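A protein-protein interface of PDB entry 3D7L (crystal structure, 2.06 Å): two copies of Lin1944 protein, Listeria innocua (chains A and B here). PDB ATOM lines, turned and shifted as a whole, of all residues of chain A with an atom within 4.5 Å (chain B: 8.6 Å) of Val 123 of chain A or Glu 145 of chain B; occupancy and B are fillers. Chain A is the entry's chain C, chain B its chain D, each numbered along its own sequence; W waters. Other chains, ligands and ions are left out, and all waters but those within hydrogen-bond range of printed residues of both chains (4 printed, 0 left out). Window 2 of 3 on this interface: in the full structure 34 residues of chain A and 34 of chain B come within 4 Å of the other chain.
The backbone NH (N) of Leu 74 of chain A lies within hydrogen-bond range of the side-chain carboxylate (OE2) of Glu 145 of chain B (2.9 Å).
The backbone NH of Gln 124 of chain A sits at hydrogen-bond distance from the side-chain carboxylate of Glu 145 of chain B (2.9 Å).
The backbone NH of Ser 72 of chain A is in hydrogen-bond range of the backbone carbonyl oxygen of Gln 124 of chain A, at 3.4 Å.
Pro 73 of chain A touches Glu 145 of chain B.
CD2 of Leu 74 of chain A touches O of Ala 142 of chain B, at 3.7 Å.
Met 146 of chain B touches Leu 74 of chain A (CE to CD2, 3.7 Å).
CG of Pro 147 of chain B touches CG2 of Thr 75 of chain A, at 3.8 Å.
Ile 122 of chain A touches Ile 144 of chain B.
Val 123 of chain A touches Ile 144 of chain B.
CG1 of Val 123 of chain A touches OE2 of Glu 145 of chain B, at 3.6 Å.
OG of Ser 141 of chain B touches C of Gly 125 of chain A (3.6 Å).
Glu 145 of chain B touches Gly 125 of chain A (OE1 to N, 3.9 Å).
Ala 126 of chain A touches Phe 138 of chain B (O to CD1, 3.96 Å).
Ser 72 of chain A touches none of the printed residues of chain B.
Of the printed residues of chain B, Pro 73 of chain A touches Glu 145.
Of chain B, only Ile 144 comes within 4 Å of Ile 122 of chain A.
Of chain B, only Ile 144 (3.8 Å) and Glu 145 (3.6 Å) come within 4 Å of Val 123 of chain A.
Of the printed residues of chain B, Ala 126 of chain A touches Phe 138 (3.96 Å) and Ser 141 (3.5 Å).
Of the printed residues of chain A, Phe 138 of chain B touches Ala 126.
Ala 139 of chain B touches none of the printed residues of chain A.
Of chain A, only Pro 73, Leu 74, Val 123, Gln 124 and Gly 125 come within 4 Å of Glu 145 of chain B.
Of the printed residues of chain A, Met 146 of chain B touches Leu 74 (3.7 Å).
Of the printed residues of chain A, Pro 147 of chain B touches Thr 75 (3.8 Å).
The nearest printed residue of chain B that does not touch Ala 126 of chain A is Glu 145 of chain B (4.3 Å).
Printed residues of chain B that touch a printed residue of chain A: Phe 138, Ser 141, Ala 142, Ile 144, Glu 145, Met 146 and Pro 147.
Hydrophobic or aromatic side chains of chain B within 4 Å of the printed part of chain A: Phe 138, Ile 144, Met 146 and Pro 147.
Hydrophobic or aromatic side chains of chain A that line the printed part of chain B: Leu 74 and Val 123.
Among the printed residues, no Asp or Glu carboxylate lies within 4 Å of a Lys or Arg side-chain nitrogen of the other chain.
No position is printed for both chains.
Of the 13 pairs that touch across the chains among the printed residues, none has its exchanged pair printed and touching as well.
Water W4 lies within hydrogen-bond range of the side-chain hydroxyl of Ser 141 of chain B (2.5 Å), the backbone NH of Ile 122 of chain A (3.0 Å) and the backbone carbonyl oxygen of Gly 125 of chain A (3.2 Å).
Water W2 lies within hydrogen-bond range of O of Ser 72 of chain A (2.7 Å), OE1 of Glu 145 of chain B (2.8 Å), N of Ala 126 of chain A (3.3 Å) and N of Leu 74 of chain A (3.5 Å).
Water W1 lies within hydrogen-bond range of the side-chain carboxylate of Glu 145 of chain B, the side-chain hydroxyl of Ser 141 of chain B, the backbone NH of Ala 126 of chain A and the backbone carbonyl oxygen of Ile 122 of chain A.
Water W3 lies within hydrogen-bond range of the side-chain carboxylate of Glu 145 of chain B (3.0 Å), the backbone NH of Leu 74 of chain A (3.3 Å) and the backbone NH of Thr 75 of chain A (3.4 Å).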
ATOM      1  N   SER A  72     -34.625   9.173 -17.677  1.00  0.00           N
ATOM      2  CA  SER A  72     -34.904  10.389 -16.916  1.00  0.00           C
ATOM      3  C   SER A  72     -33.754  10.720 -15.986  1.00  0.00           C
ATOM      4  O   SER A  72     -33.119   9.815 -15.470  1.00  0.00           O
ATOM      5  CB  SER A  72     -36.214  10.232 -16.125  1.00  0.00           C
ATOM      6  OG  SER A  72     -36.296  11.178 -15.072  1.00  0.00           O
ATOM      7  N   PRO A  73     -33.471  12.019 -15.777  1.00  0.00           N
ATOM      8  CA  PRO A  73     -32.543  12.343 -14.699  1.00  0.00           C
ATOM      9  C   PRO A  73     -33.014  11.702 -13.399  1.00  0.00           C
ATOM     10  O   PRO A  73     -34.217  11.669 -13.126  1.00  0.00           O
ATOM     11  CB  PRO A  73     -32.614  13.868 -14.603  1.00  0.00           C
ATOM     12  CG  PRO A  73     -33.048  14.318 -15.967  1.00  0.00           C
ATOM     13  CD  PRO A  73     -33.941  13.221 -16.492  1.00  0.00           C
ATOM     14  N   LEU A  74     -32.066  11.167 -12.632  1.00  0.00           N
ATOM     15  CA  LEU A  74     -32.360  10.460 -11.394  1.00  0.00           C
ATOM     16  C   LEU A  74     -33.263  11.261 -10.445  1.00  0.00           C
ATOM     17  O   LEU A  74     -34.248  10.718  -9.919  1.00  0.00           O
ATOM     18  CB  LEU A  74     -31.067  10.075 -10.688  1.00  0.00           C
ATOM     19  CG  LEU A  74     -31.204   9.489  -9.291  1.00  0.00           C
ATOM     20  CD1 LEU A  74     -31.762   8.078  -9.358  1.00  0.00           C
ATOM     21  CD2 LEU A  74     -29.867   9.520  -8.592  1.00  0.00           C
ATOM     22  N   THR A  75     -32.941  12.546 -10.251  1.00  0.00           N
ATOM     23  CA  THR A  75     -33.685  13.395  -9.318  1.00  0.00           C
ATOM     24  C   THR A  75     -35.084  13.783  -9.809  1.00  0.00           C
ATOM     25  O   THR A  75     -35.826  14.458  -9.093  1.00  0.00           O
ATOM     26  CB  THR A  75     -32.924  14.690  -8.971  1.00  0.00           C
ATOM     27  OG1 THR A  75     -32.749  15.468 -10.163  1.00  0.00           O
ATOM     28  CG2 THR A  75     -31.568  14.369  -8.293  1.00  0.00           C
ATOM     29  N   ILE A 122     -24.580   5.773 -17.461  1.00  0.00           N
ATOM     30  CA  ILE A 122     -24.662   7.115 -18.016  1.00  0.00           C
ATOM     31  C   ILE A 122     -25.785   7.887 -17.325  1.00  0.00           C
ATOM     32  O   ILE A 122     -26.733   7.277 -16.830  1.00  0.00           O
ATOM     33  CB  ILE A 122     -24.964   7.109 -19.541  1.00  0.00           C
ATOM     34  CG1 ILE A 122     -26.206   6.260 -19.872  1.00  0.00           C
ATOM     35  CG2 ILE A 122     -23.729   6.687 -20.324  1.00  0.00           C
ATOM     36  CD1 ILE A 122     -27.006   6.775 -21.079  1.00  0.00           C
ATOM     37  N   VAL A 123     -25.676   9.213 -17.310  1.00  0.00           N
ATOM     38  CA  VAL A 123     -26.755  10.083 -16.840  1.00  0.00           C
ATOM     39  C   VAL A 123     -28.041   9.752 -17.622  1.00  0.00           C
ATOM     40  O   VAL A 123     -28.013   9.610 -18.850  1.00  0.00           O
ATOM     41  CB  VAL A 123     -26.354  11.572 -16.929  1.00  0.00           C
ATOM     42  CG1 VAL A 123     -27.514  12.515 -16.604  1.00  0.00           C
ATOM     43  CG2 VAL A 123     -25.198  11.847 -15.967  1.00  0.00           C
ATOM     44  N   GLN A 124     -29.142   9.624 -16.871  1.00  0.00           N
ATOM     45  CA  GLN A 124     -30.485   9.282 -17.356  1.00  0.00           C
ATOM     46  C   GLN A 124     -30.701   7.785 -17.425  1.00  0.00           C
ATOM     47  O   GLN A 124     -31.811   7.314 -17.672  1.00  0.00           O
ATOM     48  CB  GLN A 124     -30.869   9.998 -18.669  1.00  0.00           C
ATOM     49  CG  GLN A 124     -30.894  11.519 -18.501  1.00  0.00           C
ATOM     50  CD  GLN A 124     -31.834  12.233 -19.457  1.00  0.00           C
ATOM     51  OE1 GLN A 124     -32.828  11.680 -19.892  1.00  0.00           O
ATOM     52  NE2 GLN A 124     -31.535  13.484 -19.752  1.00  0.00           N
ATOM     53  N   GLY A 125     -29.648   7.038 -17.149  1.00  0.00           N
ATOM     54  CA  GLY A 125     -29.658   5.619 -17.413  1.00  0.00           C
ATOM     55  C   GLY A 125     -29.980   4.687 -16.254  1.00  0.00           C
ATOM     56  O   GLY A 125     -29.947   3.490 -16.446  1.00  0.00           O
ATOM     57  N   ALA A 126     -30.303   5.212 -15.064  1.00  0.00           N
ATOM     58  CA  ALA A 126     -30.510   4.351 -13.879  1.00  0.00           C
ATOM     59  C   ALA A 126     -31.615   3.314 -14.068  1.00  0.00           C
ATOM     60  O   ALA A 126     -31.501   2.168 -13.600  1.00  0.00           O
ATOM     61  CB  ALA A 126     -30.796   5.176 -12.684  1.00  0.00           C
ATOM     62  N   ILE B 101     -34.103  10.900  -1.526  1.00  0.00           N
ATOM     63  CA  ILE B 101     -32.948  11.789  -1.778  1.00  0.00           C
ATOM     64  C   ILE B 101     -33.098  13.136  -1.062  1.00  0.00           C
ATOM     65  O   ILE B 101     -32.134  13.670  -0.491  1.00  0.00           O
ATOM     66  CB  ILE B 101     -32.668  11.979  -3.306  1.00  0.00           C
ATOM     67  CG1 ILE B 101     -32.340  10.640  -3.975  1.00  0.00           C
ATOM     68  CG2 ILE B 101     -31.507  12.948  -3.542  1.00  0.00           C
ATOM     69  CD1 ILE B 101     -32.476  10.650  -5.512  1.00  0.00           C
ATOM     70  N   PHE B 138     -29.059  -0.728 -10.459  1.00  0.00           N
ATOM     71  CA  PHE B 138     -29.648   0.594 -10.133  1.00  0.00           C
ATOM     72  C   PHE B 138     -28.687   1.461  -9.317  1.00  0.00           C
ATOM     73  O   PHE B 138     -28.414   2.599  -9.675  1.00  0.00           O
ATOM     74  CB  PHE B 138     -30.983   0.480  -9.363  1.00  0.00           C
ATOM     75  CG  PHE B 138     -31.508   1.820  -8.853  1.00  0.00           C
ATOM     76  CD1 PHE B 138     -32.131   2.722  -9.732  1.00  0.00           C
ATOM     77  CD2 PHE B 138     -31.338   2.202  -7.510  1.00  0.00           C
ATOM     78  CE1 PHE B 138     -32.602   3.978  -9.275  1.00  0.00           C
ATOM     79  CE2 PHE B 138     -31.789   3.450  -7.041  1.00  0.00           C
ATOM     80  CZ  PHE B 138     -32.432   4.347  -7.926  1.00  0.00           C
ATOM     81  N   ALA B 139     -28.183   0.903  -8.231  1.00  0.00           N
ATOM     82  CA  ALA B 139     -27.251   1.588  -7.316  1.00  0.00           C
ATOM     83  C   ALA B 139     -25.941   2.031  -7.986  1.00  0.00           C
ATOM     84  O   ALA B 139     -25.481   3.160  -7.771  1.00  0.00           O
ATOM     85  CB  ALA B 139     -26.945   0.688  -6.118  1.00  0.00           C
ATOM     86  N   LYS B 140     -25.347   1.135  -8.790  1.00  0.00           N
ATOM     87  CA  LYS B 140     -24.128   1.457  -9.546  1.00  0.00           C
ATOM     88  C   LYS B 140     -24.374   2.657 -10.465  1.00  0.00           C
ATOM     89  O   LYS B 140     -23.581   3.606 -10.458  1.00  0.00           O
ATOM     90  CB  LYS B 140     -23.630   0.252 -10.348  1.00  0.00           C
ATOM     91  CG  LYS B 140     -22.274   0.477 -11.020  1.00  0.00           C
ATOM     92  CD  LYS B 140     -21.842  -0.743 -11.827  1.00  0.00           C
ATOM     93  CE  LYS B 140     -20.531  -0.493 -12.597  1.00  0.00           C
ATOM     94  NZ  LYS B 140     -19.424  -0.182 -11.664  1.00  0.00           N
ATOM     95  N   SER B 141     -25.484   2.638 -11.212  1.00  0.00           N
ATOM     96  CA  SER B 141     -25.846   3.759 -12.100  1.00  0.00           C
ATOM     97  C   SER B 141     -26.256   5.026 -11.346  1.00  0.00           C
ATOM     98  O   SER B 141     -25.805   6.114 -11.665  1.00  0.00           O
ATOM     99  CB  SER B 141     -26.965   3.349 -13.080  1.00  0.00           C
ATOM    100  OG  SER B 141     -27.040   4.242 -14.182  1.00  0.00           O
ATOM    101  N   ALA B 142     -27.122   4.888 -10.348  1.00  0.00           N
ATOM    102  CA  ALA B 142     -27.588   6.038  -9.552  1.00  0.00           C
ATOM    103  C   ALA B 142     -26.437   6.851  -8.926  1.00  0.00           C
ATOM    104  O   ALA B 142     -26.494   8.075  -8.897  1.00  0.00           O
ATOM    105  CB  ALA B 142     -28.551   5.580  -8.487  1.00  0.00           C
ATOM    106  N   ALA B 143     -25.391   6.151  -8.469  1.00  0.00           N
ATOM    107  CA  ALA B 143     -24.207   6.747  -7.863  1.00  0.00           C
ATOM    108  C   ALA B 143     -23.636   7.937  -8.653  1.00  0.00           C
ATOM    109  O   ALA B 143     -23.163   8.914  -8.065  1.00  0.00           O
ATOM    110  CB  ALA B 143     -23.134   5.668  -7.660  1.00  0.00           C
ATOM    111  N   ILE B 144     -23.726   7.886  -9.980  1.00  0.00           N
ATOM    112  CA  ILE B 144     -23.176   8.961 -10.807  1.00  0.00           C
ATOM    113  C   ILE B 144     -24.093  10.193 -10.953  1.00  0.00           C
ATOM    114  O   ILE B 144     -23.657  11.237 -11.448  1.00  0.00           O
ATOM    115  CB  ILE B 144     -22.774   8.437 -12.207  1.00  0.00           C
ATOM    116  CG1 ILE B 144     -24.028   8.014 -12.995  1.00  0.00           C
ATOM    117  CG2 ILE B 144     -21.744   7.290 -12.074  1.00  0.00           C
ATOM    118  CD1 ILE B 144     -23.766   7.685 -14.441  1.00  0.00           C
ATOM    119  N   GLU B 145     -25.351  10.072 -10.525  1.00  0.00           N
ATOM    120  CA  GLU B 145     -26.307  11.176 -10.609  1.00  0.00           C
ATOM    121  C   GLU B 145     -26.703  11.774  -9.254  1.00  0.00           C
ATOM    122  O   GLU B 145     -27.566  12.642  -9.193  1.00  0.00           O
ATOM    123  CB  GLU B 145     -27.576  10.740 -11.354  1.00  0.00           C
ATOM    124  CG  GLU B 145     -27.378  10.572 -12.863  1.00  0.00           C
ATOM    125  CD  GLU B 145     -28.702  10.373 -13.579  1.00  0.00           C
ATOM    126  OE1 GLU B 145     -29.010   9.204 -13.957  1.00  0.00           O
ATOM    127  OE2 GLU B 145     -29.432  11.384 -13.727  1.00  0.00           O
ATOM    128  N   MET B 146     -26.085  11.319  -8.171  1.00  0.00           N
ATOM    129  CA  MET B 146     -26.498  11.791  -6.842  1.00  0.00           C
ATOM    130  C   MET B 146     -26.151  13.252  -6.649  1.00  0.00           C
ATOM    131  O   MET B 146     -25.064  13.674  -7.025  1.00  0.00           O
ATOM    132  CB  MET B 146     -25.919  10.912  -5.733  1.00  0.00           C
ATOM    133  CG  MET B 146     -26.605   9.538  -5.676  1.00  0.00           C
ATOM    134  SD  MET B 146     -28.444   9.650  -4.920  1.00  0.00           S
ATOM    135  CE  MET B 146     -29.101   7.887  -5.352  1.00  0.00           C
ATOM    136  N   PRO B 147     -27.099  14.041  -6.117  1.00  0.00           N
ATOM    137  CA  PRO B 147     -26.805  15.450  -5.831  1.00  0.00           C
ATOM    138  C   PRO B 147     -26.137  15.611  -4.475  1.00  0.00           C
ATOM    139  O   PRO B 147     -26.195  14.680  -3.663  1.00  0.00           O
ATOM    140  CB  PRO B 147     -28.189  16.102  -5.801  1.00  0.00           C
ATOM    141  CG  PRO B 147     -29.138  14.990  -5.382  1.00  0.00           C
ATOM    142  CD  PRO B 147     -28.490  13.671  -5.761  1.00  0.00           C
ATOM    143  N   ARG B 148     -25.486  16.767  -4.259  1.00  0.00           N
ATOM    144  CA  ARG B 148     -24.991  17.172  -2.930  1.00  0.00           C
ATOM    145  C   ARG B 148     -24.032  16.171  -2.214  1.00  0.00           C
ATOM    146  O   ARG B 148     -23.962  16.110  -0.979  1.00  0.00           O
ATOM    147  CB  ARG B 148     -26.177  17.560  -2.034  1.00  0.00           C
ATOM    148  CG  ARG B 148     -27.113  18.607  -2.657  1.00  0.00           C
ATOM    149  CD  ARG B 148     -28.297  18.931  -1.754  1.00  0.00           C
ATOM    150  NE  ARG B 148     -29.327  17.877  -1.660  1.00  0.00           N
ATOM    151  CZ  ARG B 148     -29.469  17.063  -0.615  1.00  0.00           C
ATOM    152  NH1 ARG B 148     -30.455  16.171  -0.603  1.00  0.00           N
ATOM    153  NH2 ARG B 148     -28.629  17.143   0.437  1.00  0.00           N
ATOM    154  N   GLY B 149     -23.282  15.423  -3.013  1.00  0.00           N
ATOM    155  CA  GLY B 149     -22.216  14.519  -2.527  1.00  0.00           C
ATOM    156  C   GLY B 149     -22.729  13.213  -1.939  1.00  0.00           C
ATOM    157  O   GLY B 149     -21.982  12.467  -1.302  1.00  0.00           O
ATOM    158  N   ILE B 150     -24.001  12.933  -2.174  1.00  0.00           N
ATOM    159  CA  ILE B 150     -24.648  11.755  -1.642  1.00  0.00           C
ATOM    160  C   ILE B 150     -24.081  10.477  -2.265  1.00  0.00           C
ATOM    161  O   ILE B 150     -23.796  10.438  -3.464  1.00  0.00           O
ATOM    162  CB  ILE B 150     -26.167  11.846  -1.822  1.00  0.00           C
ATOM    163  CG1 ILE B 150     -26.763  12.849  -0.805  1.00  0.00           C
ATOM    164  CG2 ILE B 150     -26.809  10.485  -1.653  1.00  0.00           C
ATOM    165  CD1 ILE B 150     -28.069  13.525  -1.247  1.00  0.00           C
ATOM    166  N   ILE B 152     -24.163   6.022  -2.665  1.00  0.00           N
ATOM    167  CA  ILE B 152     -25.065   4.863  -2.642  1.00  0.00           C
ATOM    168  C   ILE B 152     -24.302   3.570  -2.941  1.00  0.00           C
ATOM    169  O   ILE B 152     -23.625   3.455  -3.975  1.00  0.00           O
ATOM    170  CB  ILE B 152     -26.303   5.045  -3.606  1.00  0.00           C
ATOM    171  CG1 ILE B 152     -27.156   3.764  -3.650  1.00  0.00           C
ATOM    172  CG2 ILE B 152     -25.838   5.421  -5.056  1.00  0.00           C
ATOM    173  CD1 ILE B 152     -28.573   3.994  -4.187  1.00  0.00           C
ATOM    174  N   THR B 195     -18.700   4.964  -3.241  1.00  0.00           N
ATOM    175  CA  THR B 195     -20.024   4.961  -3.835  1.00  0.00           C
ATOM    176  C   THR B 195     -20.052   4.064  -5.082  1.00  0.00           C
ATOM    177  O   THR B 195     -19.027   3.813  -5.695  1.00  0.00           O
ATOM    178  CB  THR B 195     -20.499   6.411  -4.166  1.00  0.00           C
ATOM    179  OG1 THR B 195     -21.920   6.417  -4.386  1.00  0.00           O
ATOM    180  CG2 THR B 195     -19.778   6.960  -5.406  1.00  0.00           C
HETATM  181  O   HOH W   1     -27.756   6.884 -13.621  1.00  0.00           O
HETATM  182  O   HOH W   2     -31.567   8.077 -14.191  1.00  0.00           O
HETATM  183  O   HOH W   3     -30.127  13.661 -11.837  1.00  0.00           O
HETATM  184  O   HOH W   4     -26.771   3.817 -16.660  1.00  0.00           O
